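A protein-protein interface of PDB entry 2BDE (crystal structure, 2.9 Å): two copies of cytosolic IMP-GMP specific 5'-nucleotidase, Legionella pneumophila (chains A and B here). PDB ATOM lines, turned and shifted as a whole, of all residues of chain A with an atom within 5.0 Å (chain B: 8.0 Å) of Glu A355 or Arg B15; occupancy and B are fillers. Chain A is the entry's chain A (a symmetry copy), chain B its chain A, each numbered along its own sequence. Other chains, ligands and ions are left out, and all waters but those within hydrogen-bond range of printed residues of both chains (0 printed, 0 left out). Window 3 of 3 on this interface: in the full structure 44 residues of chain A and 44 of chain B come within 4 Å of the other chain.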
ATOM      1  N   LYS A 351      -0.266  -8.335  25.603  1.00  0.00           N
ATOM      2  CA  LYS A 351      -1.675  -8.123  25.285  1.00  0.00           C
ATOM      3  C   LYS A 351      -2.348  -9.467  25.034  1.00  0.00           C
ATOM      4  O   LYS A 351      -3.552  -9.616  25.231  1.00  0.00           O
ATOM      5  CB  LYS A 351      -1.823  -7.266  24.031  1.00  0.00           C
ATOM      6  CG  LYS A 351      -3.260  -7.134  23.571  1.00  0.00           C
ATOM      7  CD  LYS A 351      -3.355  -6.698  22.123  1.00  0.00           C
ATOM      8  CE  LYS A 351      -4.808  -6.580  21.692  1.00  0.00           C
ATOM      9  NZ  LYS A 351      -4.963  -6.225  20.256  1.00  0.00           N
ATOM     10  N   LYS A 352      -1.561 -10.441  24.591  1.00  0.00           N
ATOM     11  CA  LYS A 352      -2.075 -11.769  24.300  1.00  0.00           C
ATOM     12  C   LYS A 352      -2.541 -12.450  25.572  1.00  0.00           C
ATOM     13  O   LYS A 352      -3.696 -12.845  25.680  1.00  0.00           O
ATOM     14  CB  LYS A 352      -0.996 -12.612  23.625  1.00  0.00           C
ATOM     15  CG  LYS A 352      -1.517 -13.865  22.947  1.00  0.00           C
ATOM     16  CD  LYS A 352      -0.437 -14.507  22.074  1.00  0.00           C
ATOM     17  CE  LYS A 352       0.043 -13.557  20.969  1.00  0.00           C
ATOM     18  NZ  LYS A 352      -1.045 -13.197  20.011  1.00  0.00           N
ATOM     19  N   GLU A 353      -1.644 -12.583  26.541  1.00  0.00           N
ATOM     20  CA  GLU A 353      -2.008 -13.224  27.798  1.00  0.00           C
ATOM     21  C   GLU A 353      -2.977 -12.367  28.618  1.00  0.00           C
ATOM     22  O   GLU A 353      -3.734 -12.885  29.434  1.00  0.00           O
ATOM     23  CB  GLU A 353      -0.745 -13.558  28.606  1.00  0.00           C
ATOM     24  CG  GLU A 353       0.241 -12.408  28.770  1.00  0.00           C
ATOM     25  CD  GLU A 353       0.156 -11.743  30.134  1.00  0.00           C
ATOM     26  OE1 GLU A 353      -0.943 -11.277  30.508  1.00  0.00           O
ATOM     27  OE2 GLU A 353       1.197 -11.682  30.830  1.00  0.00           O
ATOM     28  N   LEU A 354      -2.961 -11.059  28.386  1.00  0.00           N
ATOM     29  CA  LEU A 354      -3.850 -10.148  29.098  1.00  0.00           C
ATOM     30  C   LEU A 354      -5.257 -10.291  28.523  1.00  0.00           C
ATOM     31  O   LEU A 354      -6.239  -9.868  29.127  1.00  0.00           O
ATOM     32  CB  LEU A 354      -3.338  -8.706  28.950  1.00  0.00           C
ATOM     33  CG  LEU A 354      -4.042  -7.554  29.676  1.00  0.00           C
ATOM     34  CD1 LEU A 354      -3.084  -6.382  29.860  1.00  0.00           C
ATOM     35  CD2 LEU A 354      -5.263  -7.127  28.885  1.00  0.00           C
ATOM     36  N   GLU A 355      -5.338 -10.907  27.351  1.00  0.00           N
ATOM     37  CA  GLU A 355      -6.608 -11.124  26.670  1.00  0.00           C
ATOM     38  C   GLU A 355      -7.011 -12.574  26.928  1.00  0.00           C
ATOM     39  O   GLU A 355      -8.189 -12.893  27.085  1.00  0.00           O
ATOM     40  CB  GLU A 355      -6.423 -10.855  25.169  1.00  0.00           C
ATOM     41  CG  GLU A 355      -7.673 -10.409  24.419  1.00  0.00           C
ATOM     42  CD  GLU A 355      -7.359  -9.792  23.058  1.00  0.00           C
ATOM     43  OE1 GLU A 355      -6.713  -8.723  23.028  1.00  0.00           O
ATOM     44  OE2 GLU A 355      -7.755 -10.373  22.021  1.00  0.00           O
ATOM     45  N   GLN A 356      -6.005 -13.443  26.978  1.00  0.00           N
ATOM     46  CA  GLN A 356      -6.195 -14.862  27.245  1.00  0.00           C
ATOM     47  C   GLN A 356      -6.923 -14.992  28.573  1.00  0.00           C
ATOM     48  O   GLN A 356      -7.788 -15.843  28.739  1.00  0.00           O
ATOM     49  CB  GLN A 356      -4.829 -15.552  27.328  1.00  0.00           C
ATOM     50  CG  GLN A 356      -4.834 -16.948  27.937  1.00  0.00           C
ATOM     51  CD  GLN A 356      -5.436 -17.999  27.020  1.00  0.00           C
ATOM     52  OE1 GLN A 356      -5.444 -19.190  27.346  1.00  0.00           O
ATOM     53  NE2 GLN A 356      -5.943 -17.566  25.866  1.00  0.00           N
ATOM     54  N   LYS A 357      -6.563 -14.129  29.517  1.00  0.00           N
ATOM     55  CA  LYS A 357      -7.177 -14.135  30.834  1.00  0.00           C
ATOM     56  C   LYS A 357      -8.487 -13.358  30.830  1.00  0.00           C
ATOM     57  O   LYS A 357      -9.317 -13.530  31.717  1.00  0.00           O
ATOM     58  CB  LYS A 357      -6.211 -13.546  31.870  1.00  0.00           C
ATOM     59  CG  LYS A 357      -4.955 -14.390  32.080  1.00  0.00           C
ATOM     60  CD  LYS A 357      -4.113 -13.906  33.256  1.00  0.00           C
ATOM     61  CE  LYS A 357      -2.918 -14.826  33.480  1.00  0.00           C
ATOM     62  NZ  LYS A 357      -2.132 -14.473  34.694  1.00  0.00           N
ATOM     63  N   TYR A 358      -8.669 -12.502  29.831  1.00  0.00           N
ATOM     64  CA  TYR A 358      -9.895 -11.717  29.727  1.00  0.00           C
ATOM     65  C   TYR A 358     -11.072 -12.622  29.422  1.00  0.00           C
ATOM     66  O   TYR A 358     -12.182 -12.381  29.890  1.00  0.00           O
ATOM     67  CB  TYR A 358      -9.790 -10.686  28.615  1.00  0.00           C
ATOM     68  CG  TYR A 358     -11.115 -10.047  28.294  1.00  0.00           C
ATOM     69  CD1 TYR A 358     -11.685  -9.118  29.152  1.00  0.00           C
ATOM     70  CD2 TYR A 358     -11.798 -10.371  27.127  1.00  0.00           C
ATOM     71  CE1 TYR A 358     -12.905  -8.522  28.856  1.00  0.00           C
ATOM     72  CE2 TYR A 358     -13.019  -9.784  26.819  1.00  0.00           C
ATOM     73  CZ  TYR A 358     -13.566  -8.858  27.684  1.00  0.00           C
ATOM     74  OH  TYR A 358     -14.764  -8.261  27.367  1.00  0.00           O
ATOM     75  N   VAL A 359     -10.827 -13.644  28.606  1.00  0.00           N
ATOM     76  CA  VAL A 359     -11.870 -14.596  28.252  1.00  0.00           C
ATOM     77  C   VAL A 359     -12.006 -15.614  29.371  1.00  0.00           C
ATOM     78  O   VAL A 359     -13.114 -15.952  29.773  1.00  0.00           O
ATOM     79  CB  VAL A 359     -11.563 -15.345  26.925  1.00  0.00           C
ATOM     80  CG1 VAL A 359     -11.548 -14.370  25.765  1.00  0.00           C
ATOM     81  CG2 VAL A 359     -10.238 -16.078  27.025  1.00  0.00           C
ATOM     82  N   ILE A 384      -6.395  -3.286  28.641  1.00  0.00           N
ATOM     83  CA  ILE A 384      -6.089  -3.857  27.336  1.00  0.00           C
ATOM     84  C   ILE A 384      -6.173  -2.748  26.299  1.00  0.00           C
ATOM     85  O   ILE A 384      -5.468  -2.765  25.296  1.00  0.00           O
ATOM     86  CB  ILE A 384      -7.095  -4.974  26.965  1.00  0.00           C
ATOM     87  CG1 ILE A 384      -6.562  -5.796  25.790  1.00  0.00           C
ATOM     88  CG2 ILE A 384      -8.448  -4.358  26.599  1.00  0.00           C
ATOM     89  CD1 ILE A 384      -7.389  -7.039  25.479  1.00  0.00           C
ATOM     90  N   ILE B  12      -8.767 -13.655  11.987  1.00  0.00           N
ATOM     91  CA  ILE B  12     -10.224 -13.672  12.072  1.00  0.00           C
ATOM     92  C   ILE B  12     -10.649 -13.601  13.539  1.00  0.00           C
ATOM     93  O   ILE B  12     -10.259 -14.437  14.361  1.00  0.00           O
ATOM     94  CB  ILE B  12     -10.853 -14.926  11.404  1.00  0.00           C
ATOM     95  CG1 ILE B  12     -12.379 -14.866  11.545  1.00  0.00           C
ATOM     96  CG2 ILE B  12     -10.314 -16.213  12.033  1.00  0.00           C
ATOM     97  CD1 ILE B  12     -13.109 -16.034  10.912  1.00  0.00           C
ATOM     98  N   ASN B  13     -11.441 -12.582  13.859  1.00  0.00           N
ATOM     99  CA  ASN B  13     -11.910 -12.368  15.221  1.00  0.00           C
ATOM    100  C   ASN B  13     -13.274 -13.008  15.435  1.00  0.00           C
ATOM    101  O   ASN B  13     -14.280 -12.526  14.918  1.00  0.00           O
ATOM    102  CB  ASN B  13     -11.997 -10.868  15.498  1.00  0.00           C
ATOM    103  CG  ASN B  13     -12.270 -10.554  16.954  1.00  0.00           C
ATOM    104  OD1 ASN B  13     -12.346  -9.389  17.338  1.00  0.00           O
ATOM    105  ND2 ASN B  13     -12.416 -11.592  17.773  1.00  0.00           N
ATOM    106  N   MET B  14     -13.310 -14.088  16.205  1.00  0.00           N
ATOM    107  CA  MET B  14     -14.570 -14.772  16.454  1.00  0.00           C
ATOM    108  C   MET B  14     -15.590 -13.922  17.185  1.00  0.00           C
ATOM    109  O   MET B  14     -16.753 -14.300  17.278  1.00  0.00           O
ATOM    110  CB  MET B  14     -14.342 -16.058  17.242  1.00  0.00           C
ATOM    111  CG  MET B  14     -13.653 -17.146  16.447  1.00  0.00           C
ATOM    112  SD  MET B  14     -14.505 -17.485  14.737  1.00  0.00           S
ATOM    113  CE  MET B  14     -16.247 -18.067  15.395  1.00  0.00           C
ATOM    114  N   ARG B  15     -15.171 -12.779  17.707  1.00  0.00           N
ATOM    115  CA  ARG B  15     -16.111 -11.929  18.417  1.00  0.00           C
ATOM    116  C   ARG B  15     -16.935 -11.145  17.417  1.00  0.00           C
ATOM    117  O   ARG B  15     -18.079 -10.797  17.684  1.00  0.00           O
ATOM    118  CB  ARG B  15     -15.365 -10.983  19.350  1.00  0.00           C
ATOM    119  CG  ARG B  15     -14.423 -11.712  20.278  1.00  0.00           C
ATOM    120  CD  ARG B  15     -13.695 -10.752  21.193  1.00  0.00           C
ATOM    121  NE  ARG B  15     -12.500 -11.367  21.763  1.00  0.00           N
ATOM    122  CZ  ARG B  15     -11.644 -10.736  22.562  1.00  0.00           C
ATOM    123  NH1 ARG B  15     -11.852  -9.463  22.890  1.00  0.00           N
ATOM    124  NH2 ARG B  15     -10.579 -11.378  23.028  1.00  0.00           N
ATOM    125  N   LYS B  16     -16.355 -10.886  16.253  1.00  0.00           N
ATOM    126  CA  LYS B  16     -17.044 -10.134  15.214  1.00  0.00           C
ATOM    127  C   LYS B  16     -18.012 -10.989  14.400  1.00  0.00           C
ATOM    128  O   LYS B  16     -18.919 -10.465  13.748  1.00  0.00           O
ATOM    129  CB  LYS B  16     -16.028  -9.509  14.267  1.00  0.00           C
ATOM    130  CG  LYS B  16     -15.978  -8.002  14.314  1.00  0.00           C
ATOM    131  CD  LYS B  16     -15.404  -7.475  15.621  1.00  0.00           C
ATOM    132  CE  LYS B  16     -15.099  -5.981  15.488  1.00  0.00           C
ATOM    133  NZ  LYS B  16     -14.541  -5.351  16.721  1.00  0.00           N
ATOM    134  N   ILE B  17     -17.821 -12.302  14.432  1.00  0.00           N
ATOM    135  CA  ILE B  17     -18.680 -13.194  13.674  1.00  0.00           C
ATOM    136  C   ILE B  17     -20.014 -13.379  14.370  1.00  0.00           C
ATOM    137  O   ILE B  17     -20.079 -13.851  15.501  1.00  0.00           O
ATOM    138  CB  ILE B  17     -18.012 -14.556  13.472  1.00  0.00           C
ATOM    139  CG1 ILE B  17     -16.670 -14.364  12.772  1.00  0.00           C
ATOM    140  CG2 ILE B  17     -18.913 -15.457  12.637  1.00  0.00           C
ATOM    141  CD1 ILE B  17     -16.765 -13.650  11.435  1.00  0.00           C
ATOM    142  N   LYS B  18     -21.077 -13.006  13.668  1.00  0.00           N
ATOM    143  CA  LYS B  18     -22.421 -13.093  14.201  1.00  0.00           C
ATOM    144  C   LYS B  18     -23.197 -14.296  13.694  1.00  0.00           C
ATOM    145  O   LYS B  18     -24.247 -14.637  14.238  1.00  0.00           O
ATOM    146  CB  LYS B  18     -23.160 -11.785  13.896  1.00  0.00           C
ATOM    147  CG  LYS B  18     -22.609 -10.629  14.714  1.00  0.00           C
ATOM    148  CD  LYS B  18     -22.721  -9.274  14.032  1.00  0.00           C
ATOM    149  CE  LYS B  18     -24.087  -8.634  14.185  1.00  0.00           C
ATOM    150  NZ  LYS B  18     -24.062  -7.243  13.634  1.00  0.00           N
ATOM    151  N   LEU B  19     -22.674 -14.945  12.661  1.00  0.00           N
ATOM    152  CA  LEU B  19     -23.324 -16.120  12.092  1.00  0.00           C
ATOM    153  C   LEU B  19     -22.307 -17.097  11.532  1.00  0.00           C
ATOM    154  O   LEU B  19     -21.310 -16.702  10.924  1.00  0.00           O
ATOM    155  CB  LEU B  19     -24.275 -15.711  10.975  1.00  0.00           C
ATOM    156  CG  LEU B  19     -25.531 -14.956  11.409  1.00  0.00           C
ATOM    157  CD1 LEU B  19     -25.714 -13.731  10.528  1.00  0.00           C
ATOM    158  CD2 LEU B  19     -26.740 -15.875  11.327  1.00  0.00           C
ATOM    159  N   TYR B 201     -23.485 -17.947  23.123  1.00  0.00           N
ATOM    160  CA  TYR B 201     -22.742 -16.698  23.009  1.00  0.00           C
ATOM    161  C   TYR B 201     -23.339 -15.764  21.957  1.00  0.00           C
ATOM    162  O   TYR B 201     -22.631 -14.963  21.353  1.00  0.00           O
ATOM    163  CB  TYR B 201     -21.269 -16.969  22.691  1.00  0.00           C
ATOM    164  CG  TYR B 201     -20.435 -17.351  23.890  1.00  0.00           C
ATOM    165  CD1 TYR B 201     -19.347 -16.566  24.283  1.00  0.00           C
ATOM    166  CD2 TYR B 201     -20.716 -18.504  24.624  1.00  0.00           C
ATOM    167  CE1 TYR B 201     -18.554 -16.915  25.379  1.00  0.00           C
ATOM    168  CE2 TYR B 201     -19.928 -18.866  25.724  1.00  0.00           C
ATOM    169  CZ  TYR B 201     -18.847 -18.061  26.097  1.00  0.00           C
ATOM    170  OH  TYR B 201     -18.080 -18.393  27.194  1.00  0.00           O
ATOM    171  N   LYS B 203     -24.238 -16.371  19.123  1.00  0.00           N
ATOM    172  CA  LYS B 203     -23.839 -16.732  17.773  1.00  0.00           C
ATOM    173  C   LYS B 203     -24.908 -17.615  17.134  1.00  0.00           C
ATOM    174  O   LYS B 203     -25.295 -18.638  17.695  1.00  0.00           O
ATOM    175  CB  LYS B 203     -22.469 -17.420  17.806  1.00  0.00           C
ATOM    176  CG  LYS B 203     -21.445 -16.721  16.906  1.00  0.00           C
ATOM    177  CD  LYS B 203     -20.010 -16.879  17.397  1.00  0.00           C
ATOM    178  CE  LYS B 203     -19.728 -16.045  18.633  1.00  0.00           C
ATOM    179  NZ  LYS B 203     -19.713 -14.593  18.343  1.00  0.00           N
ATOM    180  N   GLU B 297     -19.044 -10.516   8.716  1.00  0.00           N
ATOM    181  CA  GLU B 297     -19.634 -10.953   9.984  1.00  0.00           C
ATOM    182  C   GLU B 297     -20.241 -12.347   9.845  1.00  0.00           C
ATOM    183  O   GLU B 297     -20.975 -12.815  10.716  1.00  0.00           O
ATOM    184  CB  GLU B 297     -20.720  -9.987  10.433  1.00  0.00           C
ATOM    185  CG  GLU B 297     -20.211  -8.604  10.754  1.00  0.00           C
ATOM    186  CD  GLU B 297     -21.316  -7.687  11.213  1.00  0.00           C
ATOM    187  OE1 GLU B 297     -22.300  -7.487  10.455  1.00  0.00           O
ATOM    188  OE2 GLU B 297     -21.187  -7.166  12.341  1.00  0.00           O
ATOM    189  N   SER B 441     -13.017 -21.033  22.401  1.00  0.00           N
ATOM    190  CA  SER B 441     -13.960 -20.037  22.878  1.00  0.00           C
ATOM    191  C   SER B 441     -14.601 -19.323  21.709  1.00  0.00           C
ATOM    192  O   SER B 441     -13.910 -18.814  20.833  1.00  0.00           O
ATOM    193  CB  SER B 441     -13.257 -18.993  23.740  1.00  0.00           C
ATOM    194  OG  SER B 441     -13.988 -17.767  23.740  1.00  0.00           O
ATOM    195  N   PRO B 442     -15.936 -19.267  21.684  1.00  0.00           N
ATOM    196  CA  PRO B 442     -16.636 -18.587  20.592  1.00  0.00           C
ATOM    197  C   PRO B 442     -16.246 -17.109  20.454  1.00  0.00           C
ATOM    198  O   PRO B 442     -16.676 -16.429  19.523  1.00  0.00           O
ATOM    199  CB  PRO B 442     -18.112 -18.797  20.938  1.00  0.00           C
ATOM    200  CG  PRO B 442     -18.091 -19.041  22.421  1.00  0.00           C
ATOM    201  CD  PRO B 442     -16.888 -19.896  22.610  1.00  0.00           C
ATOM    202  N   MET B 443     -15.438 -16.611  21.385  1.00  0.00           N
ATOM    203  CA  MET B 443     -14.968 -15.232  21.312  1.00  0.00           C
ATOM    204  C   MET B 443     -13.424 -15.208  21.258  1.00  0.00           C
ATOM    205  O   MET B 443     -12.772 -14.352  21.861  1.00  0.00           O
ATOM    206  CB  MET B 443     -15.500 -14.412  22.502  1.00  0.00           C
ATOM    207  CG  MET B 443     -15.051 -14.863  23.903  1.00  0.00           C
ATOM    208  SD  MET B 443     -15.726 -13.729  25.407  1.00  0.00           S
ATOM    209  CE  MET B 443     -14.661 -12.126  25.080  1.00  0.00           C
ATOM    210  N   THR B 444     -12.862 -16.164  20.515  1.00  0.00           N
ATOM    211  CA  THR B 444     -11.420 -16.310  20.320  1.00  0.00           C
ATOM    212  C   THR B 444     -10.954 -15.426  19.179  1.00  0.00           C
ATOM    213  O   THR B 444     -11.682 -15.209  18.211  1.00  0.00           O
ATOM    214  CB  THR B 444     -11.034 -17.765  19.934  1.00  0.00           C
ATOM    215  OG1 THR B 444     -11.273 -18.643  21.037  1.00  0.00           O
ATOM    216  CG2 THR B 444      -9.570 -17.856  19.543  1.00  0.00           C
ATOM    217  N   TYR B 445      -9.729 -14.926  19.281  1.00  0.00           N
ATOM    218  CA  TYR B 445      -9.181 -14.085  18.223  1.00  0.00           C
ATOM    219  C   TYR B 445      -8.068 -14.887  17.564  1.00  0.00           C
ATOM    220  O   TYR B 445      -6.967 -14.991  18.101  1.00  0.00           O
ATOM    221  CB  TYR B 445      -8.627 -12.796  18.814  1.00  0.00           C
ATOM    222  CG  TYR B 445      -8.248 -11.758  17.789  1.00  0.00           C
ATOM    223  CD1 TYR B 445      -9.073 -10.658  17.547  1.00  0.00           C
ATOM    224  CD2 TYR B 445      -7.047 -11.859  17.077  1.00  0.00           C
ATOM    225  CE1 TYR B 445      -8.711  -9.682  16.627  1.00  0.00           C
ATOM    226  CE2 TYR B 445      -6.678 -10.887  16.150  1.00  0.00           C
ATOM    227  CZ  TYR B 445      -7.513  -9.800  15.931  1.00  0.00           C
ATOM    228  OH  TYR B 445      -7.150  -8.834  15.014  1.00  0.00           O
ATOM    229  N   PHE B 446      -8.364 -15.460  16.403  1.00  0.00           N
ATOM    230  CA  PHE B 446      -7.385 -16.273  15.688  1.00  0.00           C
ATOM    231  C   PHE B 446      -6.371 -15.437  14.908  1.00  0.00           C
ATOM    232  O   PHE B 446      -6.725 -14.734  13.961  1.00  0.00           O
ATOM    233  CB  PHE B 446      -8.110 -17.250  14.755  1.00  0.00           C
ATOM    234  CG  PHE B 446      -8.790 -18.393  15.476  1.00  0.00           C
ATOM    235  CD1 PHE B 446      -8.043 -19.445  15.999  1.00  0.00           C
ATOM    236  CD2 PHE B 446     -10.174 -18.432  15.605  1.00  0.00           C
ATOM    237  CE1 PHE B 446      -8.660 -20.520  16.635  1.00  0.00           C
ATOM    238  CE2 PHE B 446     -10.807 -19.505  16.240  1.00  0.00           C
ATOM    239  CZ  PHE B 446     -10.042 -20.550  16.752  1.00  0.00           C
ATOM    240  N   ARG B 447      -5.107 -15.520  15.322  1.00  0.00           N
ATOM    241  CA  ARG B 447      -4.027 -14.780  14.674  1.00  0.00           C
ATOM    242  C   ARG B 447      -3.143 -15.736  13.871  1.00  0.00           C
ATOM    243  O   ARG B 447      -3.102 -16.936  14.145  1.00  0.00           O
ATOM    244  CB  ARG B 447      -3.174 -14.041  15.720  1.00  0.00           C
ATOM    245  CG  ARG B 447      -3.991 -13.307  16.786  1.00  0.00           C
ATOM    246  CD  ARG B 447      -3.438 -11.909  17.145  1.00  0.00           C
ATOM    247  NE  ARG B 447      -3.613 -10.942  16.054  1.00  0.00           N
ATOM    248  CZ  ARG B 447      -3.685  -9.619  16.218  1.00  0.00           C
ATOM    249  NH1 ARG B 447      -3.598  -9.090  17.437  1.00  0.00           N
ATOM    250  NH2 ARG B 447      -3.844  -8.823  15.164  1.00  0.00           N
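OE2 of Glu A355 is in salt-bridge range of NH2 of Arg B15, 3.2 Å away.
N of Arg B15 sits close to ND2 of Asn B13 (3.0 Å).
NE of Arg B15 sits at hydrogen-bond distance from O of Met B443.
N of Met B443 lies close to OG of Ser B441 (3.0 Å).
OH of Tyr B445 sits at hydrogen-bond distance from NH2 of Arg B447.
Among the printed residues, merely in contact across the chains: Lys A352 with Arg B447 (3.9 Å), Tyr A358 with Met B443 (3.3 Å) and Val A359 with Met B443 (3.9 Å).
Of chain B, only Arg B15 comes within 4 Å of Glu A355.
Of the printed residues of chain B, Lys A352 touches Arg B447.
Of the printed residues of chain B, Val A359 touches Met B443.
Printed residues of chain B within 4 Å of Tyr A358: Met B443 (3.3 Å).
Of the printed residues of chain A, Met B443 touches Tyr A358 (3.3 Å) and Val A359 (3.9 Å).
Printed residues of chain A within 4 Å of Arg B447: Lys A352.
Of the 10 printed residues of chain A, 4 touch a printed residue of chain B.
Hydrophobic or aromatic side chains of chain A within 4 Å of the printed part of chain B: Tyr A358 and Val A359.
Printed residues of chain B that touch a printed residue of chain A: Arg B15, Met B443 and Arg B447.
Hydrophobic or aromatic side chains of chain B within 4 Å of the printed part of chain A: Met B443.
Among the printed residues, Asp or Glu carboxylates within 4 Å of a Lys or Arg side-chain nitrogen of the other chain: Glu A355 with Arg B15.
No position is printed for both chains.
Of the 4 pairs that touch across the chains among the printed residues, none has its exchanged pair printed and touching as well.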
